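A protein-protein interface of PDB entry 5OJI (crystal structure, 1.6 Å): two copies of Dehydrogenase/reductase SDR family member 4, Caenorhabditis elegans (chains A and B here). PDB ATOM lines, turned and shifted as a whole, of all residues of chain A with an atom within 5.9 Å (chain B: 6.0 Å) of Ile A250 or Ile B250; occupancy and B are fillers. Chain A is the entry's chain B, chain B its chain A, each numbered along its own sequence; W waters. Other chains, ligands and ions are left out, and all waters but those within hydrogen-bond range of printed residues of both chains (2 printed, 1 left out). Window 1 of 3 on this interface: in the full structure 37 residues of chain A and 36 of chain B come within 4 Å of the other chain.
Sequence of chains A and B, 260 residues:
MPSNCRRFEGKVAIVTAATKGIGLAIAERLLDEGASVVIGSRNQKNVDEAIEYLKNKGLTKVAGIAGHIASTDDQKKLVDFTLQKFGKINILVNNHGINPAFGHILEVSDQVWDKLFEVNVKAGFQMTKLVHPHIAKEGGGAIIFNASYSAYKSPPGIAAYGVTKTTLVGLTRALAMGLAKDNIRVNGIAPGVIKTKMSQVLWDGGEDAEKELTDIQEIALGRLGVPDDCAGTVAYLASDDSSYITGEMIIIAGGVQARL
The guanidinium group of Arg B259 sits close to the guanidinium group of Arg A259 (3.5 Å).
OH of Tyr A236 lies within hydrogen-bond range of OG1 of Thr B233, at 2.7 Å.
OH of Tyr B236 sits at hydrogen-bond distance from OG1 of Thr A233, 2.7 Å away.
The backbone carbonyl oxygen (O) of Ala B190 is in hydrogen-bond range of the backbone NH (N) of Ile B252 (3.0 Å).
The backbone carbonyl oxygen (O) of Met B249 is in hydrogen-bond range of the guanidinium group (NH2) of Arg B259.
The backbone carbonyl oxygen (O) of Gly A188 lies within hydrogen-bond range of the backbone NH (N) of Ile A250.
The backbone carbonyl oxygen of Met A249 sits at hydrogen-bond distance from the guanidinium group of Arg A259, at 2.7 Å.
The backbone NH (N) of Gly A188 sits at hydrogen-bond distance from the backbone carbonyl oxygen (O) of Glu A248, at 2.8 Å.
N of Ile A252 is in hydrogen-bond range of O of Ala A190, 3.0 Å away.
CE2 of Tyr A236 touches CE2 of Tyr B236 (3.7 Å).
CG2 of Ile B250 touches OH of Tyr A236, 3.8 Å away.
Ile A245 touches Thr B233.
Ile B251 touches Ile A245 (O to CG2, 3.8 Å).
Ile A245 touches Ile B252 (CG1 to CG2, 3.999 Å).
Ile B251 touches Glu A248 (O to CG, 3.8 Å).
Ile B250 touches Ile A250.
O of Ile A251 touches CG1 of Ile B245, at 3.8 Å.
Ile A251 touches Glu B248 (O to CG, 3.9 Å).
CG1 of Ile B245 touches CG2 of Ile A252 (3.97 Å).
Of the printed residues of chain B, Ile A250 touches Tyr B236 (3.8 Å) and Ile B250 (3.8 Å).
Ile B250 touches two residues of chain A.
Of the printed residues of chain A, Arg B259 touches Arg A259.
Printed residues of chain A within 4 Å of Glu B248: Ile A251.
Of the printed residues of chain A, Tyr B236 touches Thr A233 (2.7 Å), Tyr A236 (3.7 Å) and Ile A250 (3.8 Å).
Of the printed residues of chain B, Glu A248 touches Ile B251.
The nearest printed residue of chain B that does not touch Ile A250 is Ile B245 (4.1 Å).
The nearest printed residue of chain A that does not touch Tyr B236 is Ile A252 (5.4 Å).
Of the 14 printed residues of chain B, 8 touch a printed residue of chain A.
Along chain B the printed residues that touch a printed residue of chain A span positions 233 to 259.
Of the 14 printed residues of chain A, 8 touch a printed residue of chain B.
Among the printed residues, 15 pairs touch across the chains.
Thr A233 touches Tyr B236, and with the chains exchanged Tyr A236 touches Thr B233.
Thr A233 touches Ile B245, and with the chains exchanged Ile A245 touches Thr B233.
Glu A248 touches Ile B251, and with the chains exchanged Ile A251 touches Glu B248.
Ile A250 touches its own counterpart, Ile B250.
14 positions are printed for both chains.
Water W1 lies within hydrogen-bond range of the side-chain carboxylate (OE1) of Glu A248 (2.4 Å) and the guanidinium group (NE) of Arg B259 (2.9 Å).
Water W2 lies within hydrogen-bond range of O of Met A249 (2.8 Å), O of Met B249 (2.9 Å) and NH2 of Arg B259 (3.4 Å).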
ATOM      1  N   GLY A 188     -22.486  17.802  -8.793  1.00  0.00           N
ATOM      2  CA  GLY A 188     -23.156  18.902  -9.451  1.00  0.00           C
ATOM      3  C   GLY A 188     -23.316  20.089  -8.528  1.00  0.00           C
ATOM      4  O   GLY A 188     -23.241  19.969  -7.295  1.00  0.00           O
ATOM      5  N   ILE A 189     -23.543  21.242  -9.145  1.00  0.00           N
ATOM      6  CA  ILE A 189     -23.952  22.435  -8.426  1.00  0.00           C
ATOM      7  C   ILE A 189     -25.367  22.771  -8.868  1.00  0.00           C
ATOM      8  O   ILE A 189     -25.790  22.483  -9.999  1.00  0.00           O
ATOM      9  CB  ILE A 189     -22.991  23.628  -8.633  1.00  0.00           C
ATOM     10  CG1 ILE A 189     -22.862  24.015 -10.117  1.00  0.00           C
ATOM     11  CG2 ILE A 189     -21.633  23.298  -8.017  1.00  0.00           C
ATOM     12  CD1 ILE A 189     -22.168  25.377 -10.342  1.00  0.00           C
ATOM     13  N   ALA A 190     -26.115  23.351  -7.947  1.00  0.00           N
ATOM     14  CA  ALA A 190     -27.505  23.723  -8.170  1.00  0.00           C
ATOM     15  C   ALA A 190     -27.617  25.170  -7.725  1.00  0.00           C
ATOM     16  O   ALA A 190     -28.046  25.453  -6.597  1.00  0.00           O
ATOM     17  CB  ALA A 190     -28.458  22.796  -7.413  1.00  0.00           C
ATOM     18  N   PRO A 191     -27.209  26.108  -8.577  1.00  0.00           N
ATOM     19  CA  PRO A 191     -27.200  27.511  -8.168  1.00  0.00           C
ATOM     20  C   PRO A 191     -28.604  28.071  -8.086  1.00  0.00           C
ATOM     21  O   PRO A 191     -29.521  27.630  -8.789  1.00  0.00           O
ATOM     22  CB  PRO A 191     -26.392  28.201  -9.275  1.00  0.00           C
ATOM     23  CG  PRO A 191     -25.650  27.081  -9.964  1.00  0.00           C
ATOM     24  CD  PRO A 191     -26.566  25.931  -9.891  1.00  0.00           C
ATOM     25  N   THR A 233     -16.894  26.255  -5.490  1.00  0.00           N
ATOM     26  CA  THR A 233     -17.478  24.941  -5.278  1.00  0.00           C
ATOM     27  C   THR A 233     -17.036  23.972  -6.363  1.00  0.00           C
ATOM     28  O   THR A 233     -16.702  22.809  -6.076  1.00  0.00           O
ATOM     29  CB  THR A 233     -19.002  25.053  -5.232  1.00  0.00           C
ATOM     30  OG1 THR A 233     -19.384  25.889  -4.135  1.00  0.00           O
ATOM     31  CG2 THR A 233     -19.633  23.693  -5.047  1.00  0.00           C
ATOM     32  N   TYR A 236     -13.502  22.985  -5.706  1.00  0.00           N
ATOM     33  CA  TYR A 236     -13.501  22.001  -4.630  1.00  0.00           C
ATOM     34  C   TYR A 236     -13.974  20.637  -5.130  1.00  0.00           C
ATOM     35  O   TYR A 236     -13.351  19.606  -4.842  1.00  0.00           O
ATOM     36  CB  TYR A 236     -14.379  22.520  -3.491  1.00  0.00           C
ATOM     37  CG  TYR A 236     -15.070  21.494  -2.656  1.00  0.00           C
ATOM     38  CD1 TYR A 236     -14.396  20.780  -1.690  1.00  0.00           C
ATOM     39  CD2 TYR A 236     -16.425  21.286  -2.791  1.00  0.00           C
ATOM     40  CE1 TYR A 236     -15.058  19.857  -0.892  1.00  0.00           C
ATOM     41  CE2 TYR A 236     -17.095  20.369  -2.020  1.00  0.00           C
ATOM     42  CZ  TYR A 236     -16.416  19.660  -1.071  1.00  0.00           C
ATOM     43  OH  TYR A 236     -17.103  18.757  -0.309  1.00  0.00           O
ATOM     44  N   LEU A 237     -15.068  20.609  -5.898  1.00  0.00           N
ATOM     45  CA  LEU A 237     -15.598  19.327  -6.367  1.00  0.00           C
ATOM     46  C   LEU A 237     -14.664  18.639  -7.354  1.00  0.00           C
ATOM     47  O   LEU A 237     -14.718  17.416  -7.498  1.00  0.00           O
ATOM     48  CB  LEU A 237     -16.969  19.512  -7.010  1.00  0.00           C
ATOM     49  CG  LEU A 237     -18.137  19.801  -6.063  1.00  0.00           C
ATOM     50  CD1 LEU A 237     -19.415  20.086  -6.852  1.00  0.00           C
ATOM     51  CD2 LEU A 237     -18.371  18.646  -5.099  1.00  0.00           C
ATOM     52  N   ILE A 245     -16.197  12.061  -2.281  1.00  0.00           N
ATOM     53  CA  ILE A 245     -17.532  12.583  -2.546  1.00  0.00           C
ATOM     54  C   ILE A 245     -17.875  12.344  -4.010  1.00  0.00           C
ATOM     55  O   ILE A 245     -17.172  12.833  -4.902  1.00  0.00           O
ATOM     56  CB  ILE A 245     -17.627  14.080  -2.231  1.00  0.00           C
ATOM     57  CG1 ILE A 245     -17.290  14.325  -0.759  1.00  0.00           C
ATOM     58  CG2 ILE A 245     -19.036  14.564  -2.575  1.00  0.00           C
ATOM     59  CD1 ILE A 245     -17.086  15.765  -0.412  1.00  0.00           C
ATOM     60  N   GLU A 248     -23.192  13.740  -5.543  1.00  0.00           N
ATOM     61  CA  GLU A 248     -23.830  14.777  -4.746  1.00  0.00           C
ATOM     62  C   GLU A 248     -24.078  16.049  -5.544  1.00  0.00           C
ATOM     63  O   GLU A 248     -23.368  16.370  -6.496  1.00  0.00           O
ATOM     64  CB  GLU A 248     -22.994  15.122  -3.512  1.00  0.00           C
ATOM     65  CG  GLU A 248     -22.925  13.997  -2.457  1.00  0.00           C
ATOM     66  CD  GLU A 248     -24.286  13.395  -2.113  1.00  0.00           C
ATOM     67  OE1 GLU A 248     -25.251  14.171  -1.903  1.00  0.00           O
ATOM     68  OE2 GLU A 248     -24.384  12.142  -2.054  1.00  0.00           O
ATOM     69  N   MET A 249     -25.133  16.747  -5.143  1.00  0.00           N
ATOM     70  CA  MET A 249     -25.484  18.075  -5.606  1.00  0.00           C
ATOM     71  C   MET A 249     -25.279  19.066  -4.466  1.00  0.00           C
ATOM     72  O   MET A 249     -25.687  18.806  -3.333  1.00  0.00           O
ATOM     73  CB  MET A 249     -26.946  18.100  -6.030  1.00  0.00           C
ATOM     74  CG  MET A 249     -27.292  17.241  -7.219  1.00  0.00           C
ATOM     75  SD  MET A 249     -26.479  17.762  -8.749  1.00  0.00           S
ATOM     76  CE  MET A 249     -26.690  19.495  -8.604  1.00  0.00           C
ATOM     77  N   ILE A 250     -24.654  20.201  -4.756  1.00  0.00           N
ATOM     78  CA  ILE A 250     -24.504  21.269  -3.775  1.00  0.00           C
ATOM     79  C   ILE A 250     -25.333  22.453  -4.238  1.00  0.00           C
ATOM     80  O   ILE A 250     -25.115  22.979  -5.335  1.00  0.00           O
ATOM     81  CB  ILE A 250     -23.034  21.664  -3.579  1.00  0.00           C
ATOM     82  CG1 ILE A 250     -22.260  20.470  -3.018  1.00  0.00           C
ATOM     83  CG2 ILE A 250     -22.940  22.898  -2.648  1.00  0.00           C
ATOM     84  CD1 ILE A 250     -20.793  20.710  -2.837  1.00  0.00           C
ATOM     85  N   ILE A 251     -26.277  22.872  -3.397  1.00  0.00           N
ATOM     86  CA  ILE A 251     -27.123  24.017  -3.704  1.00  0.00           C
ATOM     87  C   ILE A 251     -26.377  25.293  -3.347  1.00  0.00           C
ATOM     88  O   ILE A 251     -25.864  25.439  -2.226  1.00  0.00           O
ATOM     89  CB  ILE A 251     -28.462  23.922  -2.960  1.00  0.00           C
ATOM     90  CG1 ILE A 251     -29.237  22.712  -3.478  1.00  0.00           C
ATOM     91  CG2 ILE A 251     -29.274  25.220  -3.141  1.00  0.00           C
ATOM     92  CD1 ILE A 251     -30.587  22.547  -2.886  1.00  0.00           C
ATOM     93  N   ILE A 252     -26.317  26.214  -4.301  1.00  0.00           N
ATOM     94  CA  ILE A 252     -25.591  27.473  -4.138  1.00  0.00           C
ATOM     95  C   ILE A 252     -26.590  28.595  -4.358  1.00  0.00           C
ATOM     96  O   ILE A 252     -26.643  29.205  -5.436  1.00  0.00           O
ATOM     97  CB  ILE A 252     -24.404  27.579  -5.110  1.00  0.00           C
ATOM     98  CG1 ILE A 252     -23.571  26.301  -5.074  1.00  0.00           C
ATOM     99  CG2 ILE A 252     -23.559  28.828  -4.779  1.00  0.00           C
ATOM    100  CD1 ILE A 252     -22.399  26.302  -6.043  1.00  0.00           C
ATOM    101  N   ARG A 259     -34.692  21.132  -0.028  1.00  0.00           N
ATOM    102  CA  ARG A 259     -34.571  19.726   0.337  1.00  0.00           C
ATOM    103  C   ARG A 259     -33.814  19.632   1.652  1.00  0.00           C
ATOM    104  O   ARG A 259     -33.135  20.572   2.064  1.00  0.00           O
ATOM    105  CB  ARG A 259     -33.850  18.909  -0.738  1.00  0.00           C
ATOM    106  CG  ARG A 259     -32.497  19.485  -1.089  1.00  0.00           C
ATOM    107  CD  ARG A 259     -31.435  18.418  -1.179  1.00  0.00           C
ATOM    108  NE  ARG A 259     -30.095  19.004  -1.248  1.00  0.00           N
ATOM    109  CZ  ARG A 259     -29.065  18.425  -1.855  1.00  0.00           C
ATOM    110  NH1 ARG A 259     -29.213  17.256  -2.461  1.00  0.00           N
ATOM    111  NH2 ARG A 259     -27.880  19.018  -1.858  1.00  0.00           N
ATOM    112  N   GLY B 188     -23.195  21.710   7.185  1.00  0.00           N
ATOM    113  CA  GLY B 188     -22.777  20.496   7.844  1.00  0.00           C
ATOM    114  C   GLY B 188     -22.151  19.506   6.893  1.00  0.00           C
ATOM    115  O   GLY B 188     -22.305  19.582   5.668  1.00  0.00           O
ATOM    116  N   ILE B 189     -21.472  18.549   7.484  1.00  0.00           N
ATOM    117  CA  ILE B 189     -21.047  17.363   6.768  1.00  0.00           C
ATOM    118  C   ILE B 189     -21.783  16.168   7.337  1.00  0.00           C
ATOM    119  O   ILE B 189     -22.205  16.148   8.503  1.00  0.00           O
ATOM    120  CB  ILE B 189     -19.523  17.183   6.842  1.00  0.00           C
ATOM    121  CG1 ILE B 189     -19.063  16.995   8.293  1.00  0.00           C
ATOM    122  CG2 ILE B 189     -18.884  18.381   6.201  1.00  0.00           C
ATOM    123  CD1 ILE B 189     -17.604  16.603   8.416  1.00  0.00           C
ATOM    124  N   ALA B 190     -21.938  15.160   6.486  1.00  0.00           N
ATOM    125  CA  ALA B 190     -22.621  13.922   6.828  1.00  0.00           C
ATOM    126  C   ALA B 190     -21.745  12.773   6.356  1.00  0.00           C
ATOM    127  O   ALA B 190     -21.979  12.182   5.287  1.00  0.00           O
ATOM    128  CB  ALA B 190     -24.022  13.904   6.215  1.00  0.00           C
ATOM    129  N   PRO B 191     -20.708  12.444   7.122  1.00  0.00           N
ATOM    130  CA  PRO B 191     -19.776  11.403   6.684  1.00  0.00           C
ATOM    131  C   PRO B 191     -20.376  10.014   6.784  1.00  0.00           C
ATOM    132  O   PRO B 191     -21.203   9.720   7.652  1.00  0.00           O
ATOM    133  CB  PRO B 191     -18.585  11.559   7.639  1.00  0.00           C
ATOM    134  CG  PRO B 191     -18.751  12.905   8.272  1.00  0.00           C
ATOM    135  CD  PRO B 191     -20.214  13.151   8.318  1.00  0.00           C
ATOM    136  N   THR B 233     -13.644  19.400   2.947  1.00  0.00           N
ATOM    137  CA  THR B 233     -15.009  19.908   2.877  1.00  0.00           C
ATOM    138  C   THR B 233     -15.276  20.939   3.968  1.00  0.00           C
ATOM    139  O   THR B 233     -15.881  21.987   3.707  1.00  0.00           O
ATOM    140  CB  THR B 233     -15.996  18.753   2.984  1.00  0.00           C
ATOM    141  OG1 THR B 233     -15.809  17.854   1.888  1.00  0.00           O
ATOM    142  CG2 THR B 233     -17.443  19.260   2.954  1.00  0.00           C
ATOM    143  N   TYR B 236     -13.548  24.095   3.014  1.00  0.00           N
ATOM    144  CA  TYR B 236     -14.345  24.761   1.992  1.00  0.00           C
ATOM    145  C   TYR B 236     -15.571  25.437   2.602  1.00  0.00           C
ATOM    146  O   TYR B 236     -15.848  26.612   2.327  1.00  0.00           O
ATOM    147  CB  TYR B 236     -14.730  23.732   0.931  1.00  0.00           C
ATOM    148  CG  TYR B 236     -15.999  23.996   0.182  1.00  0.00           C
ATOM    149  CD1 TYR B 236     -16.073  24.963  -0.811  1.00  0.00           C
ATOM    150  CD2 TYR B 236     -17.119  23.225   0.436  1.00  0.00           C
ATOM    151  CE1 TYR B 236     -17.253  25.157  -1.517  1.00  0.00           C
ATOM    152  CE2 TYR B 236     -18.266  23.404  -0.249  1.00  0.00           C
ATOM    153  CZ  TYR B 236     -18.343  24.369  -1.216  1.00  0.00           C
ATOM    154  OH  TYR B 236     -19.545  24.496  -1.864  1.00  0.00           O
ATOM    155  N   LEU B 237     -16.320  24.715   3.439  1.00  0.00           N
ATOM    156  CA  LEU B 237     -17.542  25.293   4.001  1.00  0.00           C
ATOM    157  C   LEU B 237     -17.264  26.481   4.925  1.00  0.00           C
ATOM    158  O   LEU B 237     -18.118  27.366   5.055  1.00  0.00           O
ATOM    159  CB  LEU B 237     -18.329  24.226   4.748  1.00  0.00           C
ATOM    160  CG  LEU B 237     -19.072  23.213   3.876  1.00  0.00           C
ATOM    161  CD1 LEU B 237     -19.645  22.100   4.765  1.00  0.00           C
ATOM    162  CD2 LEU B 237     -20.168  23.849   3.048  1.00  0.00           C
ATOM    163  N   ILE B 245     -23.407  29.874   0.329  1.00  0.00           N
ATOM    164  CA  ILE B 245     -23.951  28.568   0.693  1.00  0.00           C
ATOM    165  C   ILE B 245     -24.218  28.563   2.190  1.00  0.00           C
ATOM    166  O   ILE B 245     -23.297  28.775   2.992  1.00  0.00           O
ATOM    167  CB  ILE B 245     -22.993  27.427   0.334  1.00  0.00           C
ATOM    168  CG1 ILE B 245     -22.738  27.381  -1.176  1.00  0.00           C
ATOM    169  CG2 ILE B 245     -23.571  26.102   0.836  1.00  0.00           C
ATOM    170  CD1 ILE B 245     -21.518  26.556  -1.562  1.00  0.00           C
ATOM    171  N   GLU B 248     -26.839  23.920   4.220  1.00  0.00           N
ATOM    172  CA  GLU B 248     -26.689  22.718   3.423  1.00  0.00           C
ATOM    173  C   GLU B 248     -25.857  21.676   4.155  1.00  0.00           C
ATOM    174  O   GLU B 248     -25.046  21.990   5.027  1.00  0.00           O
ATOM    175  CB  GLU B 248     -26.067  23.064   2.063  1.00  0.00           C
ATOM    176  CG  GLU B 248     -26.930  24.059   1.242  1.00  0.00           C
ATOM    177  CD  GLU B 248     -28.343  23.541   0.959  1.00  0.00           C
ATOM    178  OE1 GLU B 248     -28.495  22.336   0.693  1.00  0.00           O
ATOM    179  OE2 GLU B 248     -29.311  24.334   1.012  1.00  0.00           O
ATOM    180  N   MET B 249     -26.109  20.422   3.801  1.00  0.00           N
ATOM    181  CA  MET B 249     -25.394  19.260   4.289  1.00  0.00           C
ATOM    182  C   MET B 249     -24.660  18.649   3.099  1.00  0.00           C
ATOM    183  O   MET B 249     -25.242  18.508   2.019  1.00  0.00           O
ATOM    184  CB  MET B 249     -26.383  18.251   4.866  1.00  0.00           C
ATOM    185  CG  MET B 249     -27.126  18.684   6.101  1.00  0.00           C
ATOM    186  SD  MET B 249     -26.043  18.926   7.528  1.00  0.00           S
ATOM    187  CE  MET B 249     -25.014  17.527   7.327  1.00  0.00           C
ATOM    188  N   ILE B 250     -23.386  18.312   3.272  1.00  0.00           N
ATOM    189  CA  ILE B 250     -22.645  17.600   2.242  1.00  0.00           C
ATOM    190  C   ILE B 250     -22.386  16.182   2.737  1.00  0.00           C
ATOM    191  O   ILE B 250     -21.797  15.983   3.806  1.00  0.00           O
ATOM    192  CB  ILE B 250     -21.344  18.329   1.876  1.00  0.00           C
ATOM    193  CG1 ILE B 250     -21.659  19.700   1.266  1.00  0.00           C
ATOM    194  CG2 ILE B 250     -20.517  17.493   0.901  1.00  0.00           C
ATOM    195  CD1 ILE B 250     -20.427  20.531   0.941  1.00  0.00           C
ATOM    196  N   ILE B 251     -22.857  15.201   1.976  1.00  0.00           N
ATOM    197  CA  ILE B 251     -22.618  13.800   2.302  1.00  0.00           C
ATOM    198  C   ILE B 251     -21.218  13.411   1.836  1.00  0.00           C
ATOM    199  O   ILE B 251     -20.847  13.631   0.672  1.00  0.00           O
ATOM    200  CB  ILE B 251     -23.704  12.906   1.678  1.00  0.00           C
ATOM    201  CG1 ILE B 251     -25.050  13.205   2.349  1.00  0.00           C
ATOM    202  CG2 ILE B 251     -23.368  11.439   1.838  1.00  0.00           C
ATOM    203  CD1 ILE B 251     -26.205  12.391   1.862  1.00  0.00           C
ATOM    204  N   ILE B 252     -20.432  12.850   2.757  1.00  0.00           N
ATOM    205  CA  ILE B 252     -19.062  12.421   2.492  1.00  0.00           C
ATOM    206  C   ILE B 252     -18.978  10.925   2.757  1.00  0.00           C
ATOM    207  O   ILE B 252     -18.501  10.486   3.815  1.00  0.00           O
ATOM    208  CB  ILE B 252     -18.053  13.207   3.353  1.00  0.00           C
ATOM    209  CG1 ILE B 252     -18.336  14.711   3.262  1.00  0.00           C
ATOM    210  CG2 ILE B 252     -16.630  12.888   2.914  1.00  0.00           C
ATOM    211  CD1 ILE B 252     -17.391  15.547   4.044  1.00  0.00           C
ATOM    212  N   ARG B 259     -30.364  10.404  -0.481  1.00  0.00           N
ATOM    213  CA  ARG B 259     -31.280  11.495  -0.794  1.00  0.00           C
ATOM    214  C   ARG B 259     -30.915  12.052  -2.162  1.00  0.00           C
ATOM    215  O   ARG B 259     -29.803  11.845  -2.652  1.00  0.00           O
ATOM    216  CB  ARG B 259     -31.226  12.597   0.267  1.00  0.00           C
ATOM    217  CG  ARG B 259     -29.823  13.145   0.473  1.00  0.00           C
ATOM    218  CD  ARG B 259     -29.780  14.658   0.408  1.00  0.00           C
ATOM    219  NE  ARG B 259     -28.409  15.187   0.347  1.00  0.00           N
ATOM    220  CZ  ARG B 259     -28.045  16.366   0.840  1.00  0.00           C
ATOM    221  NH1 ARG B 259     -28.935  17.133   1.453  1.00  0.00           N
ATOM    222  NH2 ARG B 259     -26.794  16.783   0.734  1.00  0.00           N
HETATM  223  O   HOH W   1     -27.342  13.090  -1.366  1.00  0.00           O
HETATM  224  O   HOH W   2     -24.519  18.826  -0.792  1.00  0.00           O
